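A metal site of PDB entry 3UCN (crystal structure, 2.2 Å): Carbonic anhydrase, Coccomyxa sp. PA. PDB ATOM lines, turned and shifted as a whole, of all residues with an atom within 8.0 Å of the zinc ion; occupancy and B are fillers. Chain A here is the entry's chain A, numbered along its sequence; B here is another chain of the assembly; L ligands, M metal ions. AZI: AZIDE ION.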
ATOM      1  N   GLY A  46      12.322 -23.947   1.814  1.00  0.00           N
ATOM      2  CA  GLY A  46      11.199 -23.358   2.528  1.00  0.00           C
ATOM      3  C   GLY A  46      11.294 -21.848   2.495  1.00  0.00           C
ATOM      4  O   GLY A  46      12.101 -21.263   1.744  1.00  0.00           O
ATOM      5  N   CYS A  47      10.474 -21.168   3.311  1.00  0.00           N
ATOM      6  CA  CYS A  47      10.304 -19.736   3.164  1.00  0.00           C
ATOM      7  C   CYS A  47      11.315 -19.094   4.072  1.00  0.00           C
ATOM      8  O   CYS A  47      11.659 -19.658   5.126  1.00  0.00           O
ATOM      9  CB  CYS A  47       8.871 -19.344   3.533  1.00  0.00           C
ATOM     10  SG  CYS A  47       8.538 -17.524   3.219  1.00  0.00           S
ATOM     11  N   ALA A  48      11.767 -17.927   3.660  1.00  0.00           N
ATOM     12  CA  ALA A  48      12.590 -17.025   4.464  1.00  0.00           C
ATOM     13  C   ALA A  48      11.942 -16.550   5.780  1.00  0.00           C
ATOM     14  O   ALA A  48      12.611 -16.057   6.668  1.00  0.00           O
ATOM     15  CB  ALA A  48      12.961 -15.826   3.674  1.00  0.00           C
ATOM     16  N   ASP A  49      10.631 -16.593   5.847  1.00  0.00           N
ATOM     17  CA  ASP A  49       9.884 -16.241   7.097  1.00  0.00           C
ATOM     18  C   ASP A  49      10.629 -16.618   8.414  1.00  0.00           C
ATOM     19  O   ASP A  49      10.977 -17.784   8.652  1.00  0.00           O
ATOM     20  CB  ASP A  49       8.525 -16.958   7.072  1.00  0.00           C
ATOM     21  CG  ASP A  49       7.592 -16.457   8.189  1.00  0.00           C
ATOM     22  OD1 ASP A  49       7.711 -16.942   9.342  1.00  0.00           O
ATOM     23  OD2 ASP A  49       6.739 -15.573   7.922  1.00  0.00           O
ATOM     24  N   SER A  50      10.813 -15.638   9.277  1.00  0.00           N
ATOM     25  CA  SER A  50      11.515 -15.878  10.589  1.00  0.00           C
ATOM     26  C   SER A  50      10.919 -16.932  11.527  1.00  0.00           C
ATOM     27  O   SER A  50      11.536 -17.256  12.528  1.00  0.00           O
ATOM     28  CB  SER A  50      11.587 -14.591  11.391  1.00  0.00           C
ATOM     29  OG  SER A  50      10.266 -14.220  11.761  1.00  0.00           O
ATOM     30  N   ARG A  51       9.739 -17.450  11.259  1.00  0.00           N
ATOM     31  CA  ARG A  51       9.223 -18.428  12.203  1.00  0.00           C
ATOM     32  C   ARG A  51       9.471 -19.844  11.815  1.00  0.00           C
ATOM     33  O   ARG A  51       8.971 -20.752  12.477  1.00  0.00           O
ATOM     34  CB  ARG A  51       7.742 -18.213  12.474  1.00  0.00           C
ATOM     35  CG  ARG A  51       7.491 -16.762  12.917  1.00  0.00           C
ATOM     36  CD  ARG A  51       6.034 -16.432  12.653  1.00  0.00           C
ATOM     37  NE  ARG A  51       5.773 -16.181  11.231  1.00  0.00           N
ATOM     38  CZ  ARG A  51       4.555 -16.052  10.723  1.00  0.00           C
ATOM     39  NH1 ARG A  51       3.504 -16.173  11.531  1.00  0.00           N
ATOM     40  NH2 ARG A  51       4.366 -15.806   9.431  1.00  0.00           N
ATOM     41  N   VAL A  52      10.242 -20.058  10.741  1.00  0.00           N
ATOM     42  CA  VAL A  52      10.269 -21.381  10.149  1.00  0.00           C
ATOM     43  C   VAL A  52      11.692 -21.816   9.930  1.00  0.00           C
ATOM     44  O   VAL A  52      12.266 -21.590   8.837  1.00  0.00           O
ATOM     45  CB  VAL A  52       9.470 -21.532   8.782  1.00  0.00           C
ATOM     46  CG1 VAL A  52       9.147 -23.064   8.486  1.00  0.00           C
ATOM     47  CG2 VAL A  52       8.212 -20.674   8.736  1.00  0.00           C
ATOM     48  N   ASN A  70      13.804 -18.814   0.746  1.00  0.00           N
ATOM     49  CA  ASN A  70      13.568 -17.632  -0.094  1.00  0.00           C
ATOM     50  C   ASN A  70      12.143 -17.146   0.163  1.00  0.00           C
ATOM     51  O   ASN A  70      11.372 -17.849   0.833  1.00  0.00           O
ATOM     52  CB  ASN A  70      13.856 -17.910  -1.584  1.00  0.00           C
ATOM     53  CG  ASN A  70      12.866 -18.878  -2.225  1.00  0.00           C
ATOM     54  OD1 ASN A  70      11.692 -18.701  -2.104  1.00  0.00           O
ATOM     55  ND2 ASN A  70      13.380 -19.933  -2.959  1.00  0.00           N
ATOM     56  N   VAL A  71      11.802 -15.940  -0.313  1.00  0.00           N
ATOM     57  CA  VAL A  71      10.499 -15.377  -0.038  1.00  0.00           C
ATOM     58  C   VAL A  71       9.401 -16.195  -0.779  1.00  0.00           C
ATOM     59  O   VAL A  71       9.279 -16.152  -1.992  1.00  0.00           O
ATOM     60  CB  VAL A  71      10.485 -13.899  -0.423  1.00  0.00           C
ATOM     61  CG1 VAL A  71       9.099 -13.351  -0.353  1.00  0.00           C
ATOM     62  CG2 VAL A  71      11.410 -13.137   0.515  1.00  0.00           C
ATOM     63  N   GLY A  72       8.600 -16.930  -0.041  1.00  0.00           N
ATOM     64  CA  GLY A  72       7.584 -17.739  -0.678  1.00  0.00           C
ATOM     65  C   GLY A  72       7.902 -19.178  -0.974  1.00  0.00           C
ATOM     66  O   GLY A  72       7.105 -19.848  -1.635  1.00  0.00           O
ATOM     67  N   ASN A  73       9.090 -19.657  -0.586  1.00  0.00           N
ATOM     68  CA  ASN A  73       9.527 -21.030  -0.978  1.00  0.00           C
ATOM     69  C   ASN A  73       9.318 -21.447  -2.469  1.00  0.00           C
ATOM     70  O   ASN A  73       8.728 -22.519  -2.771  1.00  0.00           O
ATOM     71  CB  ASN A  73       8.986 -22.122  -0.004  1.00  0.00           C
ATOM     72  CG  ASN A  73       7.486 -22.080   0.196  1.00  0.00           C
ATOM     73  OD1 ASN A  73       7.002 -21.402   1.123  1.00  0.00           O
ATOM     74  ND2 ASN A  73       6.738 -22.723  -0.700  1.00  0.00           N
ATOM     75  N   CYS A 101       8.681 -27.096   1.660  1.00  0.00           N
ATOM     76  CA  CYS A 101       7.836 -26.776   2.754  1.00  0.00           C
ATOM     77  C   CYS A 101       7.258 -25.366   2.608  1.00  0.00           C
ATOM     78  O   CYS A 101       7.965 -24.396   2.412  1.00  0.00           O
ATOM     79  CB  CYS A 101       8.689 -26.911   4.003  1.00  0.00           C
ATOM     80  SG  CYS A 101       7.933 -26.429   5.585  1.00  0.00           S
ATOM     81  N   GLY A 102       5.945 -25.235   2.740  1.00  0.00           N
ATOM     82  CA  GLY A 102       5.358 -23.885   2.837  1.00  0.00           C
ATOM     83  C   GLY A 102       4.811 -23.763   4.233  1.00  0.00           C
ATOM     84  O   GLY A 102       4.972 -24.694   5.055  1.00  0.00           O
ATOM     85  N   HIS A 103       4.176 -22.634   4.537  1.00  0.00           N
ATOM     86  CA  HIS A 103       3.638 -22.479   5.828  1.00  0.00           C
ATOM     87  C   HIS A 103       2.451 -21.496   5.850  1.00  0.00           C
ATOM     88  O   HIS A 103       2.396 -20.501   5.036  1.00  0.00           O
ATOM     89  CB  HIS A 103       4.726 -21.926   6.742  1.00  0.00           C
ATOM     90  CG  HIS A 103       5.089 -20.523   6.404  1.00  0.00           C
ATOM     91  ND1 HIS A 103       4.620 -19.447   7.116  1.00  0.00           N
ATOM     92  CD2 HIS A 103       5.807 -19.997   5.357  1.00  0.00           C
ATOM     93  CE1 HIS A 103       5.081 -18.320   6.597  1.00  0.00           C
ATOM     94  NE2 HIS A 103       5.799 -18.633   5.521  1.00  0.00           N
ATOM     95  N   TYR A 104       1.529 -21.705   6.800  1.00  0.00           N
ATOM     96  CA  TYR A 104       0.375 -20.825   6.876  1.00  0.00           C
ATOM     97  C   TYR A 104       0.854 -19.473   7.329  1.00  0.00           C
ATOM     98  O   TYR A 104       1.913 -19.361   7.942  1.00  0.00           O
ATOM     99  CB  TYR A 104      -0.727 -21.403   7.784  1.00  0.00           C
ATOM    100  CG  TYR A 104      -1.254 -22.722   7.201  1.00  0.00           C
ATOM    101  CD1 TYR A 104      -0.971 -23.961   7.804  1.00  0.00           C
ATOM    102  CD2 TYR A 104      -1.999 -22.725   6.019  1.00  0.00           C
ATOM    103  CE1 TYR A 104      -1.450 -25.163   7.254  1.00  0.00           C
ATOM    104  CE2 TYR A 104      -2.505 -23.910   5.480  1.00  0.00           C
ATOM    105  CZ  TYR A 104      -2.218 -25.113   6.104  1.00  0.00           C
ATOM    106  OH  TYR A 104      -2.676 -26.246   5.505  1.00  0.00           O
ATOM    107  N   ASN A 105       0.071 -18.450   7.023  1.00  0.00           N
ATOM    108  CA  ASN A 105       0.377 -17.103   7.396  1.00  0.00           C
ATOM    109  C   ASN A 105       1.630 -16.608   6.664  1.00  0.00           C
ATOM    110  O   ASN A 105       2.347 -15.713   7.124  1.00  0.00           O
ATOM    111  CB  ASN A 105       0.445 -16.958   8.906  1.00  0.00           C
ATOM    112  CG  ASN A 105       0.412 -15.527   9.353  1.00  0.00           C
ATOM    113  OD1 ASN A 105       1.404 -15.015   9.842  1.00  0.00           O
ATOM    114  ND2 ASN A 105      -0.730 -14.847   9.152  1.00  0.00           N
ATOM    115  N   CYS A 106       1.876 -17.212   5.495  1.00  0.00           N
ATOM    116  CA  CYS A 106       2.919 -16.798   4.574  1.00  0.00           C
ATOM    117  C   CYS A 106       2.610 -15.447   3.876  1.00  0.00           C
ATOM    118  O   CYS A 106       1.705 -15.335   3.030  1.00  0.00           O
ATOM    119  CB  CYS A 106       3.136 -17.929   3.565  1.00  0.00           C
ATOM    120  SG  CYS A 106       4.475 -17.507   2.468  1.00  0.00           S
ATOM    121  N   GLY A 107       3.351 -14.437   4.231  1.00  0.00           N
ATOM    122  CA  GLY A 107       3.179 -13.086   3.622  1.00  0.00           C
ATOM    123  C   GLY A 107       3.440 -12.995   2.102  1.00  0.00           C
ATOM    124  O   GLY A 107       2.883 -12.127   1.410  1.00  0.00           O
ATOM    125  N   ALA A 108       4.279 -13.887   1.553  1.00  0.00           N
ATOM    126  CA  ALA A 108       4.536 -13.921   0.146  1.00  0.00           C
ATOM    127  C   ALA A 108       3.249 -14.372  -0.536  1.00  0.00           C
ATOM    128  O   ALA A 108       2.883 -13.879  -1.629  1.00  0.00           O
ATOM    129  CB  ALA A 108       5.663 -14.959  -0.143  1.00  0.00           C
ATOM    130  N   CYS A 109       2.592 -15.350   0.084  1.00  0.00           N
ATOM    131  CA  CYS A 109       1.423 -15.919  -0.529  1.00  0.00           C
ATOM    132  C   CYS A 109       0.241 -14.963  -0.449  1.00  0.00           C
ATOM    133  O   CYS A 109      -0.612 -14.959  -1.335  1.00  0.00           O
ATOM    134  CB  CYS A 109       1.056 -17.261   0.116  1.00  0.00           C
ATOM    135  SG  CYS A 109       2.002 -18.620  -0.551  1.00  0.00           S
ATOM    136  N   LYS A 110       0.170 -14.151   0.585  1.00  0.00           N
ATOM    137  CA  LYS A 110      -0.783 -13.036   0.642  1.00  0.00           C
ATOM    138  C   LYS A 110      -0.518 -11.933  -0.389  1.00  0.00           C
ATOM    139  O   LYS A 110      -1.467 -11.442  -1.039  1.00  0.00           O
ATOM    140  CB  LYS A 110      -0.866 -12.412   2.063  1.00  0.00           C
ATOM    141  CG  LYS A 110      -1.775 -11.212   2.104  1.00  0.00           C
ATOM    142  CD  LYS A 110      -2.144 -10.813   3.515  1.00  0.00           C
ATOM    143  CE  LYS A 110      -3.714 -10.685   3.659  1.00  0.00           C
ATOM    144  NZ  LYS A 110      -4.035  -9.768   4.845  1.00  0.00           N
ATOM    145  N   TRP A 150      -6.176 -17.224   1.420  1.00  0.00           N
ATOM    146  CA  TRP A 150      -4.830 -17.282   1.926  1.00  0.00           C
ATOM    147  C   TRP A 150      -4.386 -18.722   2.298  1.00  0.00           C
ATOM    148  O   TRP A 150      -3.439 -19.241   1.705  1.00  0.00           O
ATOM    149  CB  TRP A 150      -4.693 -16.339   3.100  1.00  0.00           C
ATOM    150  CG  TRP A 150      -3.311 -16.014   3.460  1.00  0.00           C
ATOM    151  CD1 TRP A 150      -2.138 -16.472   2.864  1.00  0.00           C
ATOM    152  CD2 TRP A 150      -2.895 -15.175   4.540  1.00  0.00           C
ATOM    153  NE1 TRP A 150      -1.048 -15.923   3.492  1.00  0.00           N
ATOM    154  CE2 TRP A 150      -1.478 -15.147   4.537  1.00  0.00           C
ATOM    155  CE3 TRP A 150      -3.606 -14.417   5.492  1.00  0.00           C
ATOM    156  CZ2 TRP A 150      -0.754 -14.394   5.443  1.00  0.00           C
ATOM    157  CZ3 TRP A 150      -2.874 -13.661   6.418  1.00  0.00           C
ATOM    158  CH2 TRP A 150      -1.452 -13.651   6.384  1.00  0.00           C
ATOM    159  N   VAL A 154      -1.459 -21.037   0.084  1.00  0.00           N
ATOM    160  CA  VAL A 154      -0.325 -21.735   0.685  1.00  0.00           C
ATOM    161  C   VAL A 154      -0.195 -23.181   0.179  1.00  0.00           C
ATOM    162  O   VAL A 154       0.857 -23.578  -0.384  1.00  0.00           O
ATOM    163  CB  VAL A 154      -0.364 -21.610   2.241  1.00  0.00           C
ATOM    164  CG1 VAL A 154       0.575 -22.630   2.928  1.00  0.00           C
ATOM    165  CG2 VAL A 154      -0.012 -20.171   2.699  1.00  0.00           C
ATOM    166  N   ASN A 157       0.469 -23.499  -3.636  1.00  0.00           N
ATOM    167  CA  ASN A 157       1.858 -23.142  -3.899  1.00  0.00           C
ATOM    168  C   ASN A 157       2.797 -24.314  -3.589  1.00  0.00           C
ATOM    169  O   ASN A 157       3.633 -24.632  -4.405  1.00  0.00           O
ATOM    170  CB  ASN A 157       2.278 -21.846  -3.209  1.00  0.00           C
ATOM    171  CG  ASN A 157       3.622 -21.415  -3.643  1.00  0.00           C
ATOM    172  OD1 ASN A 157       3.900 -21.351  -4.864  1.00  0.00           O
ATOM    173  ND2 ASN A 157       4.513 -21.138  -2.664  1.00  0.00           N
ATOM    174  N   PRO A 190       2.851 -21.849  11.871  1.00  0.00           N
ATOM    175  CA  PRO A 190       3.638 -21.124  12.892  1.00  0.00           C
ATOM    176  C   PRO A 190       3.004 -21.087  14.292  1.00  0.00           C
ATOM    177  O   PRO A 190       3.749 -21.062  15.321  1.00  0.00           O
ATOM    178  CB  PRO A 190       3.787 -19.690  12.321  1.00  0.00           C
ATOM    179  CG  PRO A 190       3.446 -19.801  10.879  1.00  0.00           C
ATOM    180  CD  PRO A 190       2.524 -21.023  10.712  1.00  0.00           C
ATOM    181  N   GLN B  38       4.969 -11.616  12.480  1.00  0.00           N
ATOM    182  CA  GLN B  38       6.390 -11.742  12.795  1.00  0.00           C
ATOM    183  C   GLN B  38       6.973 -10.353  12.876  1.00  0.00           C
ATOM    184  O   GLN B  38       6.625  -9.507  12.062  1.00  0.00           O
ATOM    185  CB  GLN B  38       7.119 -12.577  11.716  1.00  0.00           C
ATOM    186  CG  GLN B  38       7.183 -11.924  10.322  1.00  0.00           C
ATOM    187  CD  GLN B  38       7.950 -12.744   9.274  1.00  0.00           C
ATOM    188  OE1 GLN B  38       9.017 -13.343   9.560  1.00  0.00           O
ATOM    189  NE2 GLN B  38       7.425 -12.739   8.044  1.00  0.00           N
ATOM    190  N   PHE B  66      14.943 -13.473  10.171  1.00  0.00           N
ATOM    191  CA  PHE B  66      14.451 -13.817   8.812  1.00  0.00           C
ATOM    192  C   PHE B  66      15.679 -14.331   7.987  1.00  0.00           C
ATOM    193  O   PHE B  66      16.773 -13.711   8.019  1.00  0.00           O
ATOM    194  CB  PHE B  66      13.862 -12.526   8.252  1.00  0.00           C
ATOM    195  CG  PHE B  66      13.071 -12.677   6.965  1.00  0.00           C
ATOM    196  CD1 PHE B  66      11.698 -12.629   6.997  1.00  0.00           C
ATOM    197  CD2 PHE B  66      13.711 -12.679   5.702  1.00  0.00           C
ATOM    198  CE1 PHE B  66      10.932 -12.624   5.837  1.00  0.00           C
ATOM    199  CE2 PHE B  66      12.957 -12.696   4.503  1.00  0.00           C
ATOM    200  CZ  PHE B  66      11.575 -12.671   4.563  1.00  0.00           C
ATOM    201  N   TYR B  88      12.121  -6.931   1.292  1.00  0.00           N
ATOM    202  CA  TYR B  88      10.983  -7.227   2.150  1.00  0.00           C
ATOM    203  C   TYR B  88      11.285  -7.013   3.617  1.00  0.00           C
ATOM    204  O   TYR B  88      10.415  -6.525   4.354  1.00  0.00           O
ATOM    205  CB  TYR B  88      10.552  -8.638   1.923  1.00  0.00           C
ATOM    206  CG  TYR B  88       9.250  -9.042   2.589  1.00  0.00           C
ATOM    207  CD1 TYR B  88       8.019  -8.612   2.077  1.00  0.00           C
ATOM    208  CD2 TYR B  88       9.248  -9.878   3.707  1.00  0.00           C
ATOM    209  CE1 TYR B  88       6.796  -9.008   2.686  1.00  0.00           C
ATOM    210  CE2 TYR B  88       8.017 -10.280   4.327  1.00  0.00           C
ATOM    211  CZ  TYR B  88       6.809  -9.832   3.815  1.00  0.00           C
ATOM    212  OH  TYR B  88       5.593 -10.214   4.399  1.00  0.00           O
HETATM  213  N1  AZI L   1       6.395 -15.507   4.401  1.00  0.00           N
HETATM  214  N2  AZI L   1       7.034 -14.651   4.728  1.00  0.00           N
HETATM  215  N3  AZI L   1       7.758 -13.806   5.083  1.00  0.00           N
HETATM  216 ZN    ZN M   1       6.348 -17.297   3.905  1.00  0.00          ZN
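The backbone NH (N) of Asp 49 sits close to the side-chain sulfur (SG) of Cys 47. The backbone NH of Gly 72 lies close to the side-chain sulfur of Cys 47 (3.3 Å). SG of Cys 47 lies close to O of Asn 70 (3.7 Å). The side-chain sulfur (SG) of Cys 106 sits close to the backbone NH (N) of Ala 108, at 3.7 Å. The backbone NH (N) of Cys 109 sits close to the side-chain sulfur (SG) of Cys 106, 3.7 Å away. The backbone carbonyl oxygen (O) of Cys 106 sits at hydrogen-bond distance from the indole nitrogen (NE1) of Trp 150, 2.9 Å away. The guanidinium group (NE) of Arg 51 lies within salt-bridge range of the side-chain carboxylate (OD1) of Asp 49 (2.8 Å). The side-chain carboxylate (OD2) of Asp 49 is in hydrogen-bond range of the side-chain amide nitrogen (NE2) of Gln 38 of chain B (2.9 Å).
Asp 49 touches the zinc ion (CB to ZN, 3.9 Å). Of the 28 residues printed, 4 come within 4 Å of the zinc ion. The nearest printed residue that does not touch the zinc ion is Gly 107 (4.2 Å).
The zinc ion is bound by a nitrogen (N1) of the ligand, a ring nitrogen (NE2) of His 103, the side-chain sulfur of Cys 47 and the side-chain sulfur of Cys 106. The zinc ion has four donor atoms within binding distance.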
